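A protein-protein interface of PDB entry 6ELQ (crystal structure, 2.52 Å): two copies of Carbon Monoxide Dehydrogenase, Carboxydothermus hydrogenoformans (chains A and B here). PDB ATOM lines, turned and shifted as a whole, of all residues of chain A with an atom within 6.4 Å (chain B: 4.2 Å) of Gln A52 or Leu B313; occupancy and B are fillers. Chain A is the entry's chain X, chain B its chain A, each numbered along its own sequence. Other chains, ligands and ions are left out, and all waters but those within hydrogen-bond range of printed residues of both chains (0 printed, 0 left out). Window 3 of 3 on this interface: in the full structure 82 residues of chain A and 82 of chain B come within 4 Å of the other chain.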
ATOM      1  N   CYS A  50     -20.770  24.289  25.573  1.00  0.00           N
ATOM      2  CA  CYS A  50     -21.846  25.072  24.987  1.00  0.00           C
ATOM      3  C   CYS A  50     -22.710  24.141  24.153  1.00  0.00           C
ATOM      4  O   CYS A  50     -22.280  23.056  23.756  1.00  0.00           O
ATOM      5  CB  CYS A  50     -21.318  26.235  24.137  1.00  0.00           C
ATOM      6  SG  CYS A  50     -20.902  25.793  22.443  1.00  0.00           S
ATOM      7  N   VAL A  51     -23.943  24.585  23.885  1.00  0.00           N
ATOM      8  CA  VAL A  51     -24.914  23.765  23.163  1.00  0.00           C
ATOM      9  C   VAL A  51     -24.644  23.704  21.666  1.00  0.00           C
ATOM     10  O   VAL A  51     -25.417  23.078  20.930  1.00  0.00           O
ATOM     11  CB  VAL A  51     -26.334  24.290  23.467  1.00  0.00           C
ATOM     12  CG1 VAL A  51     -27.392  23.237  23.159  1.00  0.00           C
ATOM     13  CG2 VAL A  51     -26.430  24.712  24.924  1.00  0.00           C
ATOM     14  N   GLN A  52     -23.570  24.330  21.183  1.00  0.00           N
ATOM     15  CA  GLN A  52     -23.149  24.068  19.813  1.00  0.00           C
ATOM     16  C   GLN A  52     -22.448  22.725  19.685  1.00  0.00           C
ATOM     17  O   GLN A  52     -22.441  22.142  18.596  1.00  0.00           O
ATOM     18  CB  GLN A  52     -22.223  25.176  19.301  1.00  0.00           C
ATOM     19  CG  GLN A  52     -22.858  26.557  19.236  1.00  0.00           C
ATOM     20  CD  GLN A  52     -22.059  27.529  18.384  1.00  0.00           C
ATOM     21  OE1 GLN A  52     -22.339  27.706  17.199  1.00  0.00           O
ATOM     22  NE2 GLN A  52     -21.058  28.164  18.986  1.00  0.00           N
ATOM     23  N   GLY A  53     -21.872  22.224  20.775  1.00  0.00           N
ATOM     24  CA  GLY A  53     -21.169  20.966  20.763  1.00  0.00           C
ATOM     25  C   GLY A  53     -22.099  19.770  20.732  1.00  0.00           C
ATOM     26  O   GLY A  53     -23.312  19.904  20.538  1.00  0.00           O
ATOM     27  N   PRO A  54     -21.549  18.565  20.948  1.00  0.00           N
ATOM     28  CA  PRO A  54     -20.150  18.307  21.317  1.00  0.00           C
ATOM     29  C   PRO A  54     -19.147  18.543  20.187  1.00  0.00           C
ATOM     30  O   PRO A  54     -19.462  18.328  19.018  1.00  0.00           O
ATOM     31  CB  PRO A  54     -20.155  16.820  21.709  1.00  0.00           C
ATOM     32  CG  PRO A  54     -21.596  16.433  21.828  1.00  0.00           C
ATOM     33  CD  PRO A  54     -22.329  17.321  20.887  1.00  0.00           C
ATOM     34  N   CYS A  55     -17.951  18.994  20.555  1.00  0.00           N
ATOM     35  CA  CYS A  55     -16.834  19.147  19.635  1.00  0.00           C
ATOM     36  C   CYS A  55     -15.706  18.233  20.080  1.00  0.00           C
ATOM     37  O   CYS A  55     -15.401  18.148  21.274  1.00  0.00           O
ATOM     38  CB  CYS A  55     -16.328  20.594  19.590  1.00  0.00           C
ATOM     39  SG  CYS A  55     -17.608  21.847  19.435  1.00  0.00           S
ATOM     40  N   ILE A  68     -15.959  24.190  17.436  1.00  0.00           N
ATOM     41  CA  ILE A  68     -16.759  25.093  16.614  1.00  0.00           C
ATOM     42  C   ILE A  68     -16.435  26.545  16.945  1.00  0.00           C
ATOM     43  O   ILE A  68     -16.386  27.405  16.056  1.00  0.00           O
ATOM     44  CB  ILE A  68     -18.256  24.783  16.794  1.00  0.00           C
ATOM     45  CG1 ILE A  68     -18.548  23.348  16.350  1.00  0.00           C
ATOM     46  CG2 ILE A  68     -19.111  25.773  16.019  1.00  0.00           C
ATOM     47  CD1 ILE A  68     -19.989  22.924  16.543  1.00  0.00           C
ATOM     48  N   CYS A  69     -16.192  26.837  18.225  1.00  0.00           N
ATOM     49  CA  CYS A  69     -15.814  28.184  18.629  1.00  0.00           C
ATOM     50  C   CYS A  69     -14.367  28.511  18.284  1.00  0.00           C
ATOM     51  O   CYS A  69     -13.988  29.686  18.312  1.00  0.00           O
ATOM     52  CB  CYS A  69     -16.028  28.360  20.131  1.00  0.00           C
ATOM     53  SG  CYS A  69     -14.931  27.338  21.150  1.00  0.00           S
ATOM     54  N   MET A 198     -18.113  29.212  27.742  1.00  0.00           N
ATOM     55  CA  MET A 198     -17.723  29.374  26.349  1.00  0.00           C
ATOM     56  C   MET A 198     -17.210  30.785  26.084  1.00  0.00           C
ATOM     57  O   MET A 198     -17.740  31.768  26.611  1.00  0.00           O
ATOM     58  CB  MET A 198     -18.907  29.054  25.428  1.00  0.00           C
ATOM     59  CG  MET A 198     -18.616  29.238  23.939  1.00  0.00           C
ATOM     60  SD  MET A 198     -18.882  30.927  23.348  1.00  0.00           S
ATOM     61  CE  MET A 198     -17.804  30.958  21.919  1.00  0.00           C
ATOM     62  N   VAL B  27     -16.558  29.767  11.709  1.00  0.00           N
ATOM     63  CA  VAL B  27     -17.388  28.939  12.579  1.00  0.00           C
ATOM     64  C   VAL B  27     -18.215  27.957  11.759  1.00  0.00           C
ATOM     65  O   VAL B  27     -18.455  26.822  12.191  1.00  0.00           O
ATOM     66  CB  VAL B  27     -18.273  29.837  13.470  1.00  0.00           C
ATOM     67  CG1 VAL B  27     -19.113  30.784  12.622  1.00  0.00           C
ATOM     68  CG2 VAL B  27     -19.153  28.998  14.380  1.00  0.00           C
ATOM     69  N   PHE B  28     -18.644  28.360  10.560  1.00  0.00           N
ATOM     70  CA  PHE B  28     -19.396  27.454   9.700  1.00  0.00           C
ATOM     71  C   PHE B  28     -18.514  26.323   9.188  1.00  0.00           C
ATOM     72  O   PHE B  28     -18.974  25.183   9.052  1.00  0.00           O
ATOM     73  CB  PHE B  28     -20.011  28.232   8.536  1.00  0.00           C
ATOM     74  CG  PHE B  28     -20.828  29.418   8.965  1.00  0.00           C
ATOM     75  CD1 PHE B  28     -22.170  29.273   9.284  1.00  0.00           C
ATOM     76  CD2 PHE B  28     -20.255  30.676   9.055  1.00  0.00           C
ATOM     77  CE1 PHE B  28     -22.927  30.361   9.682  1.00  0.00           C
ATOM     78  CE2 PHE B  28     -21.007  31.768   9.454  1.00  0.00           C
ATOM     79  CZ  PHE B  28     -22.344  31.609   9.766  1.00  0.00           C
ATOM     80  N   GLN B  37     -21.978  14.860  14.753  1.00  0.00           N
ATOM     81  CA  GLN B  37     -21.592  15.041  16.144  1.00  0.00           C
ATOM     82  C   GLN B  37     -22.058  13.857  16.985  1.00  0.00           C
ATOM     83  O   GLN B  37     -23.040  13.186  16.658  1.00  0.00           O
ATOM     84  CB  GLN B  37     -22.165  16.347  16.697  1.00  0.00           C
ATOM     85  CG  GLN B  37     -21.586  17.594  16.039  1.00  0.00           C
ATOM     86  CD  GLN B  37     -22.239  18.877  16.521  1.00  0.00           C
ATOM     87  OE1 GLN B  37     -23.317  19.249  16.059  1.00  0.00           O
ATOM     88  NE2 GLN B  37     -21.585  19.561  17.452  1.00  0.00           N
ATOM     89  N   ASN B 311     -23.811  40.057  15.438  1.00  0.00           N
ATOM     90  CA  ASN B 311     -24.049  39.250  16.623  1.00  0.00           C
ATOM     91  C   ASN B 311     -22.984  38.155  16.742  1.00  0.00           C
ATOM     92  O   ASN B 311     -21.891  38.268  16.178  1.00  0.00           O
ATOM     93  CB  ASN B 311     -25.474  38.677  16.594  1.00  0.00           C
ATOM     94  CG  ASN B 311     -25.826  38.029  15.272  1.00  0.00           C
ATOM     95  OD1 ASN B 311     -24.950  37.686  14.478  1.00  0.00           O
ATOM     96  ND2 ASN B 311     -27.121  37.840  15.037  1.00  0.00           N
ATOM     97  N   PHE B 312     -23.312  37.083  17.467  1.00  0.00           N
ATOM     98  CA  PHE B 312     -22.301  36.134  17.926  1.00  0.00           C
ATOM     99  C   PHE B 312     -21.699  35.337  16.775  1.00  0.00           C
ATOM    100  O   PHE B 312     -20.472  35.239  16.652  1.00  0.00           O
ATOM    101  CB  PHE B 312     -22.915  35.198  18.964  1.00  0.00           C
ATOM    102  CG  PHE B 312     -22.125  33.944  19.200  1.00  0.00           C
ATOM    103  CD1 PHE B 312     -20.972  33.970  19.970  1.00  0.00           C
ATOM    104  CD2 PHE B 312     -22.540  32.736  18.663  1.00  0.00           C
ATOM    105  CE1 PHE B 312     -20.243  32.816  20.192  1.00  0.00           C
ATOM    106  CE2 PHE B 312     -21.815  31.579  18.880  1.00  0.00           C
ATOM    107  CZ  PHE B 312     -20.665  31.619  19.647  1.00  0.00           C
ATOM    108  N   LEU B 313     -22.544  34.751  15.924  1.00  0.00           N
ATOM    109  CA  LEU B 313     -22.038  33.813  14.927  1.00  0.00           C
ATOM    110  C   LEU B 313     -21.184  34.499  13.869  1.00  0.00           C
ATOM    111  O   LEU B 313     -20.302  33.862  13.285  1.00  0.00           O
ATOM    112  CB  LEU B 313     -23.195  33.069  14.263  1.00  0.00           C
ATOM    113  CG  LEU B 313     -22.898  31.617  13.883  1.00  0.00           C
ATOM    114  CD1 LEU B 313     -22.493  30.823  15.117  1.00  0.00           C
ATOM    115  CD2 LEU B 313     -24.097  30.980  13.202  1.00  0.00           C
ATOM    116  N   ALA B 314     -21.416  35.786  13.614  1.00  0.00           N
ATOM    117  CA  ALA B 314     -20.728  36.501  12.548  1.00  0.00           C
ATOM    118  C   ALA B 314     -19.610  37.403  13.061  1.00  0.00           C
ATOM    119  O   ALA B 314     -19.183  38.315  12.345  1.00  0.00           O
ATOM    120  CB  ALA B 314     -21.730  37.317  11.731  1.00  0.00           C
ATOM    121  N   GLN B 315     -19.121  37.163  14.282  1.00  0.00           N
ATOM    122  CA  GLN B 315     -18.070  38.011  14.836  1.00  0.00           C
ATOM    123  C   GLN B 315     -16.759  37.862  14.074  1.00  0.00           C
ATOM    124  O   GLN B 315     -15.958  38.804  14.030  1.00  0.00           O
ATOM    125  CB  GLN B 315     -17.863  37.695  16.320  1.00  0.00           C
ATOM    126  CG  GLN B 315     -17.420  36.267  16.600  1.00  0.00           C
ATOM    127  CD  GLN B 315     -17.281  35.976  18.082  1.00  0.00           C
ATOM    128  OE1 GLN B 315     -16.199  36.106  18.653  1.00  0.00           O
ATOM    129  NE2 GLN B 315     -18.380  35.576  18.714  1.00  0.00           N
ATOM    130  N   ASN B 447     -26.613  33.078  18.932  1.00  0.00           N
ATOM    131  CA  ASN B 447     -26.676  32.353  17.674  1.00  0.00           C
ATOM    132  C   ASN B 447     -26.175  30.931  17.887  1.00  0.00           C
ATOM    133  O   ASN B 447     -25.493  30.628  18.868  1.00  0.00           O
ATOM    134  CB  ASN B 447     -25.838  33.037  16.591  1.00  0.00           C
ATOM    135  CG  ASN B 447     -26.250  34.472  16.346  1.00  0.00           C
ATOM    136  OD1 ASN B 447     -25.432  35.385  16.449  1.00  0.00           O
ATOM    137  ND2 ASN B 447     -27.520  34.680  16.014  1.00  0.00           N
ATOM    138  N   ASN B 448     -26.531  30.050  16.957  1.00  0.00           N
ATOM    139  CA  ASN B 448     -26.089  28.664  17.038  1.00  0.00           C
ATOM    140  C   ASN B 448     -25.944  28.118  15.629  1.00  0.00           C
ATOM    141  O   ASN B 448     -26.921  28.079  14.875  1.00  0.00           O
ATOM    142  CB  ASN B 448     -27.068  27.814  17.850  1.00  0.00           C
ATOM    143  CG  ASN B 448     -26.474  26.482  18.266  1.00  0.00           C
ATOM    144  OD1 ASN B 448     -25.756  25.841  17.498  1.00  0.00           O
ATOM    145  ND2 ASN B 448     -26.763  26.065  19.492  1.00  0.00           N
ATOM    146  N   VAL B 449     -24.729  27.681  15.290  1.00  0.00           N
ATOM    147  CA  VAL B 449     -24.446  27.174  13.954  1.00  0.00           C
ATOM    148  C   VAL B 449     -25.341  25.993  13.594  1.00  0.00           C
ATOM    149  O   VAL B 449     -25.568  25.726  12.409  1.00  0.00           O
ATOM    150  CB  VAL B 449     -22.950  26.813  13.849  1.00  0.00           C
ATOM    151  CG1 VAL B 449     -22.643  25.552  14.643  1.00  0.00           C
ATOM    152  CG2 VAL B 449     -22.529  26.680  12.394  1.00  0.00           C
ATOM    153  N   LYS B 450     -25.881  25.287  14.593  1.00  0.00           N
ATOM    154  CA  LYS B 450     -26.874  24.253  14.326  1.00  0.00           C
ATOM    155  C   LYS B 450     -28.128  24.813  13.668  1.00  0.00           C
ATOM    156  O   LYS B 450     -28.925  24.044  13.120  1.00  0.00           O
ATOM    157  CB  LYS B 450     -27.261  23.538  15.621  1.00  0.00           C
ATOM    158  CG  LYS B 450     -26.160  22.701  16.248  1.00  0.00           C
ATOM    159  CD  LYS B 450     -26.645  22.080  17.546  1.00  0.00           C
ATOM    160  CE  LYS B 450     -25.569  21.240  18.206  1.00  0.00           C
ATOM    161  NZ  LYS B 450     -26.031  20.708  19.518  1.00  0.00           N
ATOM    162  N   HIS B 453     -28.251  30.975  10.412  1.00  0.00           N
ATOM    163  CA  HIS B 453     -27.927  32.165  11.191  1.00  0.00           C
ATOM    164  C   HIS B 453     -29.025  33.215  11.083  1.00  0.00           C
ATOM    165  O   HIS B 453     -29.328  33.700   9.988  1.00  0.00           O
ATOM    166  CB  HIS B 453     -26.588  32.738  10.731  1.00  0.00           C
ATOM    167  CG  HIS B 453     -26.266  34.074  11.322  1.00  0.00           C
ATOM    168  ND1 HIS B 453     -26.326  35.243  10.594  1.00  0.00           N
ATOM    169  CD2 HIS B 453     -25.881  34.429  12.570  1.00  0.00           C
ATOM    170  CE1 HIS B 453     -25.991  36.259  11.369  1.00  0.00           C
ATOM    171  NE2 HIS B 453     -25.715  35.792  12.572  1.00  0.00           N
ATOM    172  N   GLN B 559     -26.819  29.092  22.672  1.00  0.00           N
ATOM    173  CA  GLN B 559     -25.623  28.257  22.641  1.00  0.00           C
ATOM    174  C   GLN B 559     -24.904  28.269  23.986  1.00  0.00           C
ATOM    175  O   GLN B 559     -24.395  27.236  24.435  1.00  0.00           O
ATOM    176  CB  GLN B 559     -24.681  28.711  21.519  1.00  0.00           C
ATOM    177  CG  GLN B 559     -24.090  30.109  21.684  1.00  0.00           C
ATOM    178  CD  GLN B 559     -22.761  30.107  22.419  1.00  0.00           C
ATOM    179  OE1 GLN B 559     -22.072  29.090  22.470  1.00  0.00           O
ATOM    180  NE2 GLN B 559     -22.397  31.250  22.996  1.00  0.00           N
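The side-chain sulfur (SG) of Cys A50 lies close to the side-chain amide oxygen (OE1) of Gln B559 (3.5 Å).
The side-chain amino group (NZ) of Lys B450 is in hydrogen-bond range of the backbone carbonyl oxygen (O) of Val A51 (2.8 Å).
The backbone NH (N) of Val A51 sits at hydrogen-bond distance from the backbone carbonyl oxygen (O) of Gln B559.
NE2 of Gln B37 lies within hydrogen-bond range of O of Gln A52 (3.0 Å).
OE1 of Gln A52 sits at hydrogen-bond distance from N of Val B449, at 3.1 Å.
The backbone carbonyl oxygen (O) of Gly A53 sits at hydrogen-bond distance from the side-chain amino group (NZ) of Lys B450, at 3.0 Å.
The backbone carbonyl oxygen (O) of Pro A54 sits at hydrogen-bond distance from the side-chain amide nitrogen (NE2) of Gln B37 (2.9 Å).
SD of Met A198 sits at hydrogen-bond distance from NE2 of Gln B559, 3.5 Å away.
The backbone NH (N) of Gln A52 lies close to the side-chain sulfur (SG) of Cys A50.
N of Ile A68 sits close to SG of Cys A55.
The backbone carbonyl oxygen (O) of Phe B312 lies within hydrogen-bond range of the side-chain amide nitrogen (NE2) of Gln B315 (3.0 Å).
The backbone NH of Phe B312 is in hydrogen-bond range of the side-chain amide oxygen of Asn B447 (2.9 Å).
The backbone NH of Leu B313 lies within hydrogen-bond range of the side-chain amide oxygen of Asn B447, at 3.0 Å.
The side-chain amide oxygen (OD1) of Asn B448 is in hydrogen-bond range of the backbone NH (N) of Lys B450, at 3.0 Å.
Val A51 touches Asn B448 (O to ND2, 3.6 Å).
NE2 of Gln A52 touches CE2 of Phe B312, 3.5 Å away.
Leu B313 touches Gln A52 (CD1 to OE1, 3.8 Å).
Asn B448 touches Gln A52.
Lys B450 touches Gln A52 (CE to O, 3.3 Å).
Gln A52 touches Gln B559.
C of Gly A53 touches NE2 of Gln B37 (3.3 Å).
CD1 of Ile A68 touches NE2 of Gln B37 (3.8 Å).
Ile A68 touches Val B449 (CG2 to CG1, 3.8 Å).
Met A198 touches Phe B312.
Of chain B, only Gln B37, Phe B312, Leu B313, Asn B448, Val B449, Lys B450 and Gln B559 come within 4 Å of Gln A52.
Leu B313 touches just one residue of chain A: Gln A52 (3.8 Å).
Printed residues of chain A within 4 Å of Val B27: Ile A68 (3.6 Å).
Of the printed residues of chain A, Val B449 touches Gln A52 (3.1 Å) and Ile A68 (3.8 Å).
Of the printed residues of chain B, Met A198 touches Phe B312 (3.5 Å) and Gln B559 (3.5 Å).
Ala B314 touches none of the printed residues of chain A.
Printed residues of chain A that touch a printed residue of chain B: Cys A50, Val A51, Gln A52, Gly A53, Pro A54, Ile A68 and Met A198.
Hydrophobic or aromatic side chains of chain A within 4 Å of the printed part of chain B: Val A51, Ile A68 and Met A198.
Of the 14 printed residues of chain B, 8 touch a printed residue of chain A.
Printed residues of chain B that touch a printed residue of chain A: Val B27, Gln B37, Phe B312, Leu B313, Asn B448, Val B449, Lys B450 and Gln B559.
Hydrophobic or aromatic side chains of chain B that line the printed part of chain A: Val B27, Phe B312, Leu B313 and Val B449.
Among the printed residues, 19 pairs touch across the chains.
No position is printed for both chains.
Of the 19 pairs that touch across the chains among the printed residues, none has its exchanged pair printed and touching as well.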
